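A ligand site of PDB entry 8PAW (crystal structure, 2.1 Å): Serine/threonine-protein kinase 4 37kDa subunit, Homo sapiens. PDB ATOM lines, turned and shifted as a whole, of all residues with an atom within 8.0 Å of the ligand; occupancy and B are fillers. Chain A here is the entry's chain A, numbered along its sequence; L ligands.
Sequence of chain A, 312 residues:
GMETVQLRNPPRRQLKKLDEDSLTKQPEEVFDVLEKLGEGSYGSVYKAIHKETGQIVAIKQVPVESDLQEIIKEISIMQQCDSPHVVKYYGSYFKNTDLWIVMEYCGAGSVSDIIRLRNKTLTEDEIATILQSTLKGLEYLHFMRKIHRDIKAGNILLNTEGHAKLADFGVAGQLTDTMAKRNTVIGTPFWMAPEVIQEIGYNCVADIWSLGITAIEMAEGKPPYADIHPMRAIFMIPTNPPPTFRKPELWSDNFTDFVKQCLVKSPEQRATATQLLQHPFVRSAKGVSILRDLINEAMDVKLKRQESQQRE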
ATOM      1  N   LEU A 117     -20.576   2.670 -25.669  1.00  0.00           N
ATOM      2  CA  LEU A 117     -21.749   3.574 -25.866  1.00  0.00           C
ATOM      3  C   LEU A 117     -22.779   3.360 -24.759  1.00  0.00           C
ATOM      4  O   LEU A 117     -23.291   4.335 -24.258  1.00  0.00           O
ATOM      5  CB  LEU A 117     -22.377   3.340 -27.251  1.00  0.00           C
ATOM      6  CG  LEU A 117     -21.571   3.864 -28.446  1.00  0.00           C
ATOM      7  CD1 LEU A 117     -22.217   3.451 -29.751  1.00  0.00           C
ATOM      8  CD2 LEU A 117     -21.426   5.379 -28.378  1.00  0.00           C
ATOM      9  N   ARG A 118     -23.087   2.110 -24.400  1.00  0.00           N
ATOM     10  CA  ARG A 118     -24.107   1.801 -23.356  1.00  0.00           C
ATOM     11  C   ARG A 118     -23.471   1.918 -21.967  1.00  0.00           C
ATOM     12  O   ARG A 118     -24.211   1.854 -20.965  1.00  0.00           O
ATOM     13  CB  ARG A 118     -24.668   0.392 -23.552  1.00  0.00           C
ATOM     14  CG  ARG A 118     -25.553   0.213 -24.779  1.00  0.00           C
ATOM     15  CD  ARG A 118     -26.569  -0.894 -24.525  1.00  0.00           C
ATOM     16  NE  ARG A 118     -25.941  -2.038 -23.882  1.00  0.00           N
ATOM     17  CZ  ARG A 118     -26.528  -2.929 -23.089  1.00  0.00           C
ATOM     18  NH1 ARG A 118     -27.817  -2.847 -22.792  1.00  0.00           N
ATOM     19  NH2 ARG A 118     -25.820  -3.936 -22.601  1.00  0.00           N
ATOM     20  N   ARG A 292     -31.503  -7.079 -29.641  1.00  0.00           N
ATOM     21  CA  ARG A 292     -32.361  -6.010 -30.226  1.00  0.00           C
ATOM     22  C   ARG A 292     -32.383  -4.834 -29.245  1.00  0.00           C
ATOM     23  O   ARG A 292     -32.114  -3.693 -29.687  1.00  0.00           O
ATOM     24  CB  ARG A 292     -33.780  -6.534 -30.514  1.00  0.00           C
ATOM     25  CG  ARG A 292     -34.390  -6.160 -31.855  1.00  0.00           C
ATOM     26  CD  ARG A 292     -35.577  -7.051 -32.212  1.00  0.00           C
ATOM     27  NE  ARG A 292     -36.275  -7.608 -31.042  1.00  0.00           N
ATOM     28  CZ  ARG A 292     -37.176  -8.600 -31.067  1.00  0.00           C
ATOM     29  NH1 ARG A 292     -37.726  -8.998 -29.935  1.00  0.00           N
ATOM     30  NH2 ARG A 292     -37.521  -9.178 -32.199  1.00  0.00           N
ATOM     31  N   ASP A 293     -32.651  -5.120 -27.970  1.00  0.00           N
ATOM     32  CA  ASP A 293     -32.535  -4.150 -26.845  1.00  0.00           C
ATOM     33  C   ASP A 293     -31.179  -3.457 -26.949  1.00  0.00           C
ATOM     34  O   ASP A 293     -31.113  -2.213 -26.987  1.00  0.00           O
ATOM     35  CB  ASP A 293     -32.642  -4.822 -25.465  1.00  0.00           C
ATOM     36  CG  ASP A 293     -34.050  -4.981 -24.909  1.00  0.00           C
ATOM     37  OD1 ASP A 293     -35.000  -4.579 -25.612  1.00  0.00           O
ATOM     38  OD2 ASP A 293     -34.178  -5.517 -23.789  1.00  0.00           O
ATOM     39  N   LEU A 294     -30.121  -4.278 -26.964  1.00  0.00           N
ATOM     40  CA  LEU A 294     -28.704  -3.879 -26.914  1.00  0.00           C
ATOM     41  C   LEU A 294     -28.422  -2.916 -28.068  1.00  0.00           C
ATOM     42  O   LEU A 294     -27.879  -1.805 -27.841  1.00  0.00           O
ATOM     43  CB  LEU A 294     -27.914  -5.191 -27.037  1.00  0.00           C
ATOM     44  CG  LEU A 294     -26.405  -5.065 -27.102  1.00  0.00           C
ATOM     45  CD1 LEU A 294     -25.761  -6.135 -26.253  1.00  0.00           C
ATOM     46  CD2 LEU A 294     -25.917  -5.133 -28.528  1.00  0.00           C
ATOM     47  N   ILE A 295     -28.806  -3.299 -29.283  1.00  0.00           N
ATOM     48  CA  ILE A 295     -28.512  -2.497 -30.495  1.00  0.00           C
ATOM     49  C   ILE A 295     -29.320  -1.193 -30.459  1.00  0.00           C
ATOM     50  O   ILE A 295     -28.728  -0.161 -30.783  1.00  0.00           O
ATOM     51  CB  ILE A 295     -28.746  -3.326 -31.776  1.00  0.00           C
ATOM     52  CG1 ILE A 295     -27.488  -4.124 -32.113  1.00  0.00           C
ATOM     53  CG2 ILE A 295     -29.187  -2.452 -32.947  1.00  0.00           C
ATOM     54  CD1 ILE A 295     -27.757  -5.368 -32.877  1.00  0.00           C
ATOM     55  N   ASN A 296     -30.597  -1.248 -30.079  1.00  0.00           N
ATOM     56  CA  ASN A 296     -31.485  -0.049 -30.016  1.00  0.00           C
ATOM     57  C   ASN A 296     -30.876   0.981 -29.065  1.00  0.00           C
ATOM     58  O   ASN A 296     -30.664   2.124 -29.512  1.00  0.00           O
ATOM     59  CB  ASN A 296     -32.921  -0.423 -29.628  1.00  0.00           C
ATOM     60  CG  ASN A 296     -33.665  -1.046 -30.778  1.00  0.00           C
ATOM     61  OD1 ASN A 296     -33.435  -0.687 -31.927  1.00  0.00           O
ATOM     62  ND2 ASN A 296     -34.547  -1.987 -30.498  1.00  0.00           N
ATOM     63  N   GLU A 297     -30.555   0.567 -27.831  1.00  0.00           N
ATOM     64  CA  GLU A 297     -29.919   1.449 -26.808  1.00  0.00           C
ATOM     65  C   GLU A 297     -28.612   2.025 -27.361  1.00  0.00           C
ATOM     66  O   GLU A 297     -28.420   3.241 -27.203  1.00  0.00           O
ATOM     67  CB  GLU A 297     -29.680   0.660 -25.518  1.00  0.00           C
ATOM     68  CG  GLU A 297     -30.964   0.165 -24.881  1.00  0.00           C
ATOM     69  CD  GLU A 297     -30.725  -0.775 -23.720  1.00  0.00           C
ATOM     70  OE1 GLU A 297     -31.675  -1.466 -23.296  1.00  0.00           O
ATOM     71  OE2 GLU A 297     -29.576  -0.820 -23.249  1.00  0.00           O
ATOM     72  N   ALA A 298     -27.763   1.220 -27.997  1.00  0.00           N
ATOM     73  CA  ALA A 298     -26.449   1.649 -28.543  1.00  0.00           C
ATOM     74  C   ALA A 298     -26.618   2.716 -29.634  1.00  0.00           C
ATOM     75  O   ALA A 298     -25.778   3.644 -29.673  1.00  0.00           O
ATOM     76  CB  ALA A 298     -25.665   0.465 -29.081  1.00  0.00           C
ATOM     77  N   MET A 299     -27.611   2.558 -30.517  1.00  0.00           N
ATOM     78  CA  MET A 299     -27.941   3.477 -31.643  1.00  0.00           C
ATOM     79  C   MET A 299     -29.110   4.379 -31.229  1.00  0.00           C
ATOM     80  O   MET A 299     -29.002   5.593 -31.145  1.00  0.00           O
ATOM     81  CB  MET A 299     -28.368   2.711 -32.892  1.00  0.00           C
ATOM     82  CG  MET A 299     -27.332   1.738 -33.422  1.00  0.00           C
ATOM     83  SD  MET A 299     -27.848   1.012 -35.013  1.00  0.00           S
ATOM     84  CE  MET A 299     -29.638   0.998 -34.873  1.00  0.00           C
HETATM   85  N1  LIG L   1     -29.939   5.021 -28.652  1.00  0.00           N
HETATM   86  C1  LIG L   1     -30.993   6.068 -28.759  1.00  0.00           C
HETATM   87  C2  LIG L   1     -30.907   6.968 -27.520  1.00  0.00           C
HETATM   88  O1  LIG L   1     -30.149   6.675 -26.586  1.00  0.00           O
HETATM   89  C3  LIG L   1     -32.370   5.436 -28.963  1.00  0.00           C
HETATM   90  C4  LIG L   1     -32.790   4.373 -27.953  1.00  0.00           C
HETATM   91  O2  LIG L   1     -33.703   3.613 -28.276  1.00  0.00           O
HETATM   92  O3  LIG L   1     -32.217   4.324 -26.839  1.00  0.00           O
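The backbone carbonyl oxygen (O) of Asn 296 sits at hydrogen-bond distance from a nitrogen (N1) of the ligand.
The backbone carbonyl oxygen (O) of Glu 297 is in hydrogen-bond range of a nitrogen (N1) of the ligand (2.8 Å).
N1 of the ligand lies within hydrogen-bond range of O of Met 299 (2.7 Å).
The backbone carbonyl oxygen (O) of Arg 292 is in hydrogen-bond range of the side-chain amide nitrogen (ND2) of Asn 296 (3.1 Å).
The side-chain carboxylate (OE2) of Glu 297 is in salt-bridge range of the guanidinium group (NH1) of Arg 118 (2.7 Å).
Three residues have an atom within 4 Å of the ligand: Asn 296, Glu 297 and Met 299.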
